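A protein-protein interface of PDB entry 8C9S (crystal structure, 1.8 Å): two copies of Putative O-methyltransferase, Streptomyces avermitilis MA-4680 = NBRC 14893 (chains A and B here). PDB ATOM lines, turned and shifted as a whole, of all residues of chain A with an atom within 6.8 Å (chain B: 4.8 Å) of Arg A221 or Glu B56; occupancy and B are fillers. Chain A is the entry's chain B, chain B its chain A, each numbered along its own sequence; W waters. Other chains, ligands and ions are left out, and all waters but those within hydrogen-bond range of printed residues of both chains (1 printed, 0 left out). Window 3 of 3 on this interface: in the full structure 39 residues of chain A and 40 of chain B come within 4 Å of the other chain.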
ATOM      1  N   GLN A  58      -6.979  13.008 -14.541  1.00  0.00           N
ATOM      2  CA  GLN A  58      -6.625  13.686 -15.812  1.00  0.00           C
ATOM      3  C   GLN A  58      -7.592  14.842 -16.158  1.00  0.00           C
ATOM      4  O   GLN A  58      -7.168  15.762 -16.893  1.00  0.00           O
ATOM      5  CB  GLN A  58      -6.624  12.603 -16.896  1.00  0.00           C
ATOM      6  CG  GLN A  58      -6.098  13.078 -18.228  1.00  0.00           C
ATOM      7  CD  GLN A  58      -4.590  13.030 -18.303  1.00  0.00           C
ATOM      8  OE1 GLN A  58      -4.021  13.076 -19.389  1.00  0.00           O
ATOM      9  NE2 GLN A  58      -3.927  12.967 -17.159  1.00  0.00           N
ATOM     10  N   ARG A 159      -1.835  14.837 -26.661  1.00  0.00           N
ATOM     11  CA  ARG A 159      -1.074  16.060 -26.416  1.00  0.00           C
ATOM     12  C   ARG A 159      -0.208  15.817 -25.185  1.00  0.00           C
ATOM     13  O   ARG A 159      -0.316  14.770 -24.543  1.00  0.00           O
ATOM     14  CB  ARG A 159      -2.057  17.224 -26.266  1.00  0.00           C
ATOM     15  CG  ARG A 159      -2.965  17.084 -25.058  1.00  0.00           C
ATOM     16  CD  ARG A 159      -3.557  18.411 -24.608  1.00  0.00           C
ATOM     17  NE  ARG A 159      -4.352  19.061 -25.637  1.00  0.00           N
ATOM     18  CZ  ARG A 159      -5.664  18.932 -25.799  1.00  0.00           C
ATOM     19  NH1 ARG A 159      -6.370  18.158 -24.992  1.00  0.00           N
ATOM     20  NH2 ARG A 159      -6.273  19.602 -26.757  1.00  0.00           N
ATOM     21  N   PRO A 160       0.668  16.792 -24.865  1.00  0.00           N
ATOM     22  CA  PRO A 160       1.481  16.756 -23.666  1.00  0.00           C
ATOM     23  C   PRO A 160       0.566  16.563 -22.463  1.00  0.00           C
ATOM     24  O   PRO A 160      -0.450  17.285 -22.376  1.00  0.00           O
ATOM     25  CB  PRO A 160       2.167  18.143 -23.648  1.00  0.00           C
ATOM     26  CG  PRO A 160       2.240  18.477 -25.113  1.00  0.00           C
ATOM     27  CD  PRO A 160       0.890  18.031 -25.633  1.00  0.00           C
ATOM     28  N   GLY A 161       0.914  15.590 -21.628  1.00  0.00           N
ATOM     29  CA  GLY A 161       0.197  15.291 -20.383  1.00  0.00           C
ATOM     30  C   GLY A 161      -0.919  14.286 -20.601  1.00  0.00           C
ATOM     31  O   GLY A 161      -1.500  13.847 -19.624  1.00  0.00           O
ATOM     32  N   SER A 162      -1.207  13.886 -21.837  1.00  0.00           N
ATOM     33  CA  SER A 162      -2.111  12.736 -22.084  1.00  0.00           C
ATOM     34  C   SER A 162      -1.545  11.491 -21.392  1.00  0.00           C
ATOM     35  O   SER A 162      -0.318  11.407 -21.221  1.00  0.00           O
ATOM     36  CB  SER A 162      -2.327  12.479 -23.548  1.00  0.00           C
ATOM     37  OG  SER A 162      -3.049  13.527 -24.170  1.00  0.00           O
ATOM     38  N   LEU A 163      -2.415  10.518 -21.111  1.00  0.00           N
ATOM     39  CA  LEU A 163      -2.070   9.264 -20.422  1.00  0.00           C
ATOM     40  C   LEU A 163      -2.365   8.101 -21.358  1.00  0.00           C
ATOM     41  O   LEU A 163      -3.368   8.167 -22.056  1.00  0.00           O
ATOM     42  CB  LEU A 163      -2.945   9.195 -19.176  1.00  0.00           C
ATOM     43  CG  LEU A 163      -2.485   8.243 -18.088  1.00  0.00           C
ATOM     44  CD1 LEU A 163      -1.117   8.670 -17.534  1.00  0.00           C
ATOM     45  CD2 LEU A 163      -3.530   8.247 -16.992  1.00  0.00           C
ATOM     46  N   ILE A 164      -1.479   7.121 -21.402  1.00  0.00           N
ATOM     47  CA  ILE A 164      -1.660   5.849 -22.147  1.00  0.00           C
ATOM     48  C   ILE A 164      -1.610   4.727 -21.128  1.00  0.00           C
ATOM     49  O   ILE A 164      -0.642   4.679 -20.331  1.00  0.00           O
ATOM     50  CB  ILE A 164      -0.582   5.684 -23.217  1.00  0.00           C
ATOM     51  CG1 ILE A 164      -0.577   6.892 -24.152  1.00  0.00           C
ATOM     52  CG2 ILE A 164      -0.749   4.364 -23.952  1.00  0.00           C
ATOM     53  CD1 ILE A 164       0.612   6.963 -25.028  1.00  0.00           C
ATOM     54  N   ILE A 195       7.981   2.984 -25.129  1.00  0.00           N
ATOM     55  CA  ILE A 195       7.743   3.893 -23.980  1.00  0.00           C
ATOM     56  C   ILE A 195       9.094   4.322 -23.381  1.00  0.00           C
ATOM     57  O   ILE A 195       9.272   5.509 -23.151  1.00  0.00           O
ATOM     58  CB  ILE A 195       6.824   3.256 -22.919  1.00  0.00           C
ATOM     59  CG1 ILE A 195       5.428   3.013 -23.496  1.00  0.00           C
ATOM     60  CG2 ILE A 195       6.777   4.145 -21.691  1.00  0.00           C
ATOM     61  CD1 ILE A 195       4.574   2.077 -22.677  1.00  0.00           C
ATOM     62  N   LYS A 200       9.139  11.548 -25.677  1.00  0.00           N
ATOM     63  CA  LYS A 200       7.791  12.076 -25.326  1.00  0.00           C
ATOM     64  C   LYS A 200       7.075  11.104 -24.377  1.00  0.00           C
ATOM     65  O   LYS A 200       5.920  11.406 -24.023  1.00  0.00           O
ATOM     66  CB  LYS A 200       6.940  12.337 -26.570  1.00  0.00           C
ATOM     67  CG  LYS A 200       7.411  13.476 -27.475  1.00  0.00           C
ATOM     68  CD  LYS A 200       6.543  13.657 -28.724  1.00  0.00           C
ATOM     69  CE  LYS A 200       5.497  14.750 -28.619  1.00  0.00           C
ATOM     70  NZ  LYS A 200       4.930  14.910 -27.253  1.00  0.00           N
ATOM     71  N   LEU A 201       7.695  10.001 -23.950  1.00  0.00           N
ATOM     72  CA  LEU A 201       6.980   9.043 -23.063  1.00  0.00           C
ATOM     73  C   LEU A 201       7.773   8.744 -21.807  1.00  0.00           C
ATOM     74  O   LEU A 201       8.970   8.564 -21.872  1.00  0.00           O
ATOM     75  CB  LEU A 201       6.668   7.754 -23.809  1.00  0.00           C
ATOM     76  CG  LEU A 201       5.677   7.886 -24.968  1.00  0.00           C
ATOM     77  CD1 LEU A 201       5.625   6.575 -25.739  1.00  0.00           C
ATOM     78  CD2 LEU A 201       4.288   8.277 -24.470  1.00  0.00           C
ATOM     79  N   SER A 202       7.063   8.657 -20.698  1.00  0.00           N
ATOM     80  CA  SER A 202       7.623   8.220 -19.405  1.00  0.00           C
ATOM     81  C   SER A 202       6.614   7.296 -18.723  1.00  0.00           C
ATOM     82  O   SER A 202       5.484   7.703 -18.590  1.00  0.00           O
ATOM     83  CB  SER A 202       7.941   9.379 -18.565  1.00  0.00           C
ATOM     84  OG  SER A 202       8.488   8.894 -17.361  1.00  0.00           O
ATOM     85  N   GLY A 203       7.015   6.103 -18.308  1.00  0.00           N
ATOM     86  CA  GLY A 203       6.051   5.130 -17.780  1.00  0.00           C
ATOM     87  C   GLY A 203       6.576   4.243 -16.687  1.00  0.00           C
ATOM     88  O   GLY A 203       7.717   4.413 -16.216  1.00  0.00           O
ATOM     89  N   THR A 204       5.692   3.347 -16.273  1.00  0.00           N
ATOM     90  CA  THR A 204       5.975   2.241 -15.343  1.00  0.00           C
ATOM     91  C   THR A 204       5.073   1.069 -15.693  1.00  0.00           C
ATOM     92  O   THR A 204       4.157   1.178 -16.587  1.00  0.00           O
ATOM     93  CB  THR A 204       5.806   2.703 -13.884  1.00  0.00           C
ATOM     94  OG1 THR A 204       6.495   1.787 -13.024  1.00  0.00           O
ATOM     95  CG2 THR A 204       4.358   2.867 -13.483  1.00  0.00           C
ATOM     96  N   LEU A 219       1.512   2.078 -17.573  1.00  0.00           N
ATOM     97  CA  LEU A 219       0.928   3.429 -17.547  1.00  0.00           C
ATOM     98  C   LEU A 219       2.033   4.329 -18.069  1.00  0.00           C
ATOM     99  O   LEU A 219       3.169   4.185 -17.586  1.00  0.00           O
ATOM    100  CB  LEU A 219       0.563   3.704 -16.087  1.00  0.00           C
ATOM    101  CG  LEU A 219       0.190   5.130 -15.722  1.00  0.00           C
ATOM    102  CD1 LEU A 219      -0.879   5.678 -16.658  1.00  0.00           C
ATOM    103  CD2 LEU A 219      -0.308   5.170 -14.290  1.00  0.00           C
ATOM    104  N   ALA A 220       1.754   5.127 -19.081  1.00  0.00           N
ATOM    105  CA  ALA A 220       2.736   6.069 -19.647  1.00  0.00           C
ATOM    106  C   ALA A 220       2.099   7.448 -19.737  1.00  0.00           C
ATOM    107  O   ALA A 220       0.913   7.517 -20.054  1.00  0.00           O
ATOM    108  CB  ALA A 220       3.177   5.595 -20.998  1.00  0.00           C
ATOM    109  N   ARG A 221       2.865   8.481 -19.417  1.00  0.00           N
ATOM    110  CA  ARG A 221       2.480   9.890 -19.599  1.00  0.00           C
ATOM    111  C   ARG A 221       3.183  10.492 -20.820  1.00  0.00           C
ATOM    112  O   ARG A 221       4.400  10.286 -20.999  1.00  0.00           O
ATOM    113  CB  ARG A 221       2.887  10.648 -18.345  1.00  0.00           C
ATOM    114  CG  ARG A 221       2.118  11.932 -18.173  1.00  0.00           C
ATOM    115  CD  ARG A 221       2.233  12.352 -16.724  1.00  0.00           C
ATOM    116  NE  ARG A 221       2.990  13.563 -16.652  1.00  0.00           N
ATOM    117  CZ  ARG A 221       2.510  14.772 -16.862  1.00  0.00           C
ATOM    118  NH1 ARG A 221       1.233  14.971 -17.140  1.00  0.00           N
ATOM    119  NH2 ARG A 221       3.319  15.797 -16.744  1.00  0.00           N
ATOM    120  N   VAL A 222       2.438  11.225 -21.630  1.00  0.00           N
ATOM    121  CA  VAL A 222       3.017  12.021 -22.732  1.00  0.00           C
ATOM    122  C   VAL A 222       3.716  13.264 -22.156  1.00  0.00           C
ATOM    123  O   VAL A 222       3.080  14.067 -21.449  1.00  0.00           O
ATOM    124  CB  VAL A 222       1.983  12.359 -23.805  1.00  0.00           C
ATOM    125  CG1 VAL A 222       2.633  13.131 -24.940  1.00  0.00           C
ATOM    126  CG2 VAL A 222       1.296  11.091 -24.309  1.00  0.00           C
ATOM    127  N   LEU A 223       4.988  13.436 -22.495  1.00  0.00           N
ATOM    128  CA  LEU A 223       5.808  14.608 -22.083  1.00  0.00           C
ATOM    129  C   LEU A 223       5.872  15.628 -23.218  1.00  0.00           C
ATOM    130  O   LEU A 223       5.982  15.266 -24.398  1.00  0.00           O
ATOM    131  CB  LEU A 223       7.226  14.157 -21.721  1.00  0.00           C
ATOM    132  CG  LEU A 223       7.332  13.001 -20.733  1.00  0.00           C
ATOM    133  CD1 LEU A 223       8.776  12.527 -20.639  1.00  0.00           C
ATOM    134  CD2 LEU A 223       6.770  13.379 -19.371  1.00  0.00           C
ATOM    135  N   PRO A 224       5.901  16.930 -22.867  1.00  0.00           N
ATOM    136  CA  PRO A 224       6.210  18.016 -23.815  1.00  0.00           C
ATOM    137  C   PRO A 224       7.323  17.775 -24.849  1.00  0.00           C
ATOM    138  O   PRO A 224       8.494  17.637 -24.497  1.00  0.00           O
ATOM    139  CB  PRO A 224       6.668  19.114 -22.845  1.00  0.00           C
ATOM    140  CG  PRO A 224       5.746  18.934 -21.679  1.00  0.00           C
ATOM    141  CD  PRO A 224       5.606  17.432 -21.514  1.00  0.00           C
ATOM    142  N   GLN B  52       5.446   8.857  -8.581  1.00  0.00           N
ATOM    143  CA  GLN B  52       5.916  10.060  -9.296  1.00  0.00           C
ATOM    144  C   GLN B  52       4.914  10.384 -10.410  1.00  0.00           C
ATOM    145  O   GLN B  52       4.552  11.577 -10.571  1.00  0.00           O
ATOM    146  CB  GLN B  52       7.320   9.828  -9.843  1.00  0.00           C
ATOM    147  CG  GLN B  52       7.918  11.038 -10.560  1.00  0.00           C
ATOM    148  CD  GLN B  52       9.320  10.692 -10.998  1.00  0.00           C
ATOM    149  OE1 GLN B  52       9.534  10.165 -12.068  1.00  0.00           O
ATOM    150  NE2 GLN B  52      10.268  10.843 -10.098  1.00  0.00           N
ATOM    151  N   LEU B  53       4.537   9.391 -11.204  1.00  0.00           N
ATOM    152  CA  LEU B  53       3.610   9.604 -12.345  1.00  0.00           C
ATOM    153  C   LEU B  53       2.242  10.099 -11.852  1.00  0.00           C
ATOM    154  O   LEU B  53       1.696  11.005 -12.504  1.00  0.00           O
ATOM    155  CB  LEU B  53       3.473   8.315 -13.140  1.00  0.00           C
ATOM    156  CG  LEU B  53       4.673   7.986 -14.016  1.00  0.00           C
ATOM    157  CD1 LEU B  53       4.501   6.609 -14.599  1.00  0.00           C
ATOM    158  CD2 LEU B  53       4.852   9.030 -15.138  1.00  0.00           C
ATOM    159  N   LEU B  54       1.724   9.566 -10.744  1.00  0.00           N
ATOM    160  CA  LEU B  54       0.411   9.995 -10.185  1.00  0.00           C
ATOM    161  C   LEU B  54       0.490  11.463  -9.762  1.00  0.00           C
ATOM    162  O   LEU B  54      -0.440  12.214 -10.050  1.00  0.00           O
ATOM    163  CB  LEU B  54       0.059   9.111  -8.988  1.00  0.00           C
ATOM    164  CG  LEU B  54      -0.388   7.690  -9.327  1.00  0.00           C
ATOM    165  CD1 LEU B  54      -0.517   6.855  -8.060  1.00  0.00           C
ATOM    166  CD2 LEU B  54      -1.692   7.705 -10.104  1.00  0.00           C
ATOM    167  N   ALA B  55       1.576  11.858  -9.105  1.00  0.00           N
ATOM    168  CA  ALA B  55       1.805  13.265  -8.694  1.00  0.00           C
ATOM    169  C   ALA B  55       1.869  14.152  -9.947  1.00  0.00           C
ATOM    170  O   ALA B  55       1.226  15.246  -9.973  1.00  0.00           O
ATOM    171  CB  ALA B  55       3.055  13.344  -7.851  1.00  0.00           C
ATOM    172  N   GLU B  56       2.601  13.707 -10.964  1.00  0.00           N
ATOM    173  CA  GLU B  56       2.735  14.466 -12.238  1.00  0.00           C
ATOM    174  C   GLU B  56       1.363  14.630 -12.909  1.00  0.00           C
ATOM    175  O   GLU B  56       1.061  15.739 -13.354  1.00  0.00           O
ATOM    176  CB  GLU B  56       3.738  13.798 -13.173  1.00  0.00           C
ATOM    177  CG  GLU B  56       5.157  14.062 -12.730  1.00  0.00           C
ATOM    178  CD  GLU B  56       6.223  13.303 -13.487  1.00  0.00           C
ATOM    179  OE1 GLU B  56       5.882  12.648 -14.475  1.00  0.00           O
ATOM    180  OE2 GLU B  56       7.390  13.404 -13.089  1.00  0.00           O
ATOM    181  N   ILE B  57       0.588  13.548 -13.048  1.00  0.00           N
ATOM    182  CA  ILE B  57      -0.739  13.581 -13.721  1.00  0.00           C
ATOM    183  C   ILE B  57      -1.653  14.558 -12.974  1.00  0.00           C
ATOM    184  O   ILE B  57      -2.390  15.323 -13.610  1.00  0.00           O
ATOM    185  CB  ILE B  57      -1.322  12.162 -13.750  1.00  0.00           C
ATOM    186  CG1 ILE B  57      -0.503  11.285 -14.695  1.00  0.00           C
ATOM    187  CG2 ILE B  57      -2.794  12.199 -14.124  1.00  0.00           C
ATOM    188  CD1 ILE B  57      -0.497   9.813 -14.290  1.00  0.00           C
ATOM    189  N   GLN B  58      -1.600  14.515 -11.654  1.00  0.00           N
ATOM    190  CA  GLN B  58      -2.464  15.354 -10.801  1.00  0.00           C
ATOM    191  C   GLN B  58      -2.041  16.835 -10.896  1.00  0.00           C
ATOM    192  O   GLN B  58      -2.853  17.679 -10.580  1.00  0.00           O
ATOM    193  CB  GLN B  58      -2.415  14.834  -9.371  1.00  0.00           C
ATOM    194  CG  GLN B  58      -3.640  15.274  -8.578  1.00  0.00           C
ATOM    195  CD  GLN B  58      -3.366  16.506  -7.765  1.00  0.00           C
ATOM    196  OE1 GLN B  58      -2.274  17.097  -7.789  1.00  0.00           O
ATOM    197  NE2 GLN B  58      -4.389  16.910  -7.035  1.00  0.00           N
ATOM    198  N   GLY B  59      -0.795  17.128 -11.247  1.00  0.00           N
ATOM    199  CA  GLY B  59      -0.247  18.494 -11.259  1.00  0.00           C
ATOM    200  C   GLY B  59       0.158  18.882  -9.852  1.00  0.00           C
ATOM    201  O   GLY B  59      -0.021  20.051  -9.485  1.00  0.00           O
ATOM    202  N   ARG B  79      10.640  14.418  -6.985  1.00  0.00           N
ATOM    203  CA  ARG B  79      11.036  14.631  -8.401  1.00  0.00           C
ATOM    204  C   ARG B  79       9.846  14.990  -9.281  1.00  0.00           C
ATOM    205  O   ARG B  79      10.102  15.465 -10.375  1.00  0.00           O
ATOM    206  CB  ARG B  79      11.739  13.389  -8.928  1.00  0.00           C
ATOM    207  CG  ARG B  79      13.185  13.344  -8.461  1.00  0.00           C
ATOM    208  CD  ARG B  79      13.904  12.084  -8.856  1.00  0.00           C
ATOM    209  NE  ARG B  79      15.300  12.240  -8.533  1.00  0.00           N
ATOM    210  CZ  ARG B  79      16.209  11.291  -8.636  1.00  0.00           C
ATOM    211  NH1 ARG B  79      15.873  10.073  -9.028  1.00  0.00           N
ATOM    212  NH2 ARG B  79      17.469  11.583  -8.371  1.00  0.00           N
ATOM    213  N   ALA B  80       8.604  14.821  -8.817  1.00  0.00           N
ATOM    214  CA  ALA B  80       7.415  15.313  -9.547  1.00  0.00           C
ATOM    215  C   ALA B  80       7.245  16.824  -9.353  1.00  0.00           C
ATOM    216  O   ALA B  80       6.424  17.421 -10.064  1.00  0.00           O
ATOM    217  CB  ALA B  80       6.190  14.572  -9.085  1.00  0.00           C
HETATM  218  O   HOH W   1      -2.632  15.408 -16.140  1.00  0.00           O
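NE of Arg A221 is in salt-bridge range of OE1 of Glu B56 (3.7 Å).
The backbone carbonyl oxygen (O) of Ser A202 sits at hydrogen-bond distance from the backbone NH (N) of Arg A221. OE1 of Gln A58 lies close to O of Gly A161, at 2.6 Å. The backbone carbonyl oxygen (O) of Thr A204 lies within hydrogen-bond range of the backbone NH (N) of Leu A219, at 3.0 Å. The side-chain amide oxygen of Gln A58 is in hydrogen-bond range of the backbone NH of Leu A163 (3.5 Å).
Among the printed residues, merely in contact across the chains: Gln A58 with Ile B57 (3.3 Å), Leu A163 with Ile B57 (3.5 Å), Ser A202 with Leu B53 (3.8 Å), Gly A203 with Leu B53 (3.8 Å), Thr A204 with Leu B53 (3.9 Å) and Arg A221 with Ile B57 (3.6 Å).
Of the printed residues of chain B, Gln A58 touches Ile B57 (3.3 Å). Of the printed residues of chain B, Ser A202 touches Leu B53. Printed residues of chain B within 4 Å of Thr A204: Leu B53. Arg A221 touches two residues of chain B. Of chain A, only Arg A221 (3.6 Å) comes within 4 Å of Glu B56. The nearest residue of chain B that does not touch Arg A221 is Leu B53 (4.1 Å). The nearest residue of chain A that does not touch Glu B56 is Leu A223 (5.0 Å).
Of the 19 printed residues of chain A, 6 touch a printed residue of chain B. Printed residues of chain A that touch a printed residue of chain B: Gln A58, Leu A163, Ser A202, Gly A203, Thr A204 and Arg A221. Of the 10 printed residues of chain B, 3 touch a printed residue of chain A. Hydrophobic or aromatic side chains of chain B within 4 Å of the printed part of chain A: Leu B53 and Ile B57. Among the printed residues, 7 pairs touch across the chains. Among the printed residues, Asp or Glu carboxylates within 4 Å of a Lys or Arg side-chain nitrogen of the other chain: Arg A221 with Glu B56 (3.7 Å).
1 position is printed for both chains. Of the 7 pairs that touch across the chains among the printed residues, none has its exchanged pair printed and touching as well.
Water W1 lies within hydrogen-bond range of the backbone carbonyl oxygen of Ile B57 (2.5 Å) and the side-chain amide nitrogen of Gln A58 (2.9 Å).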
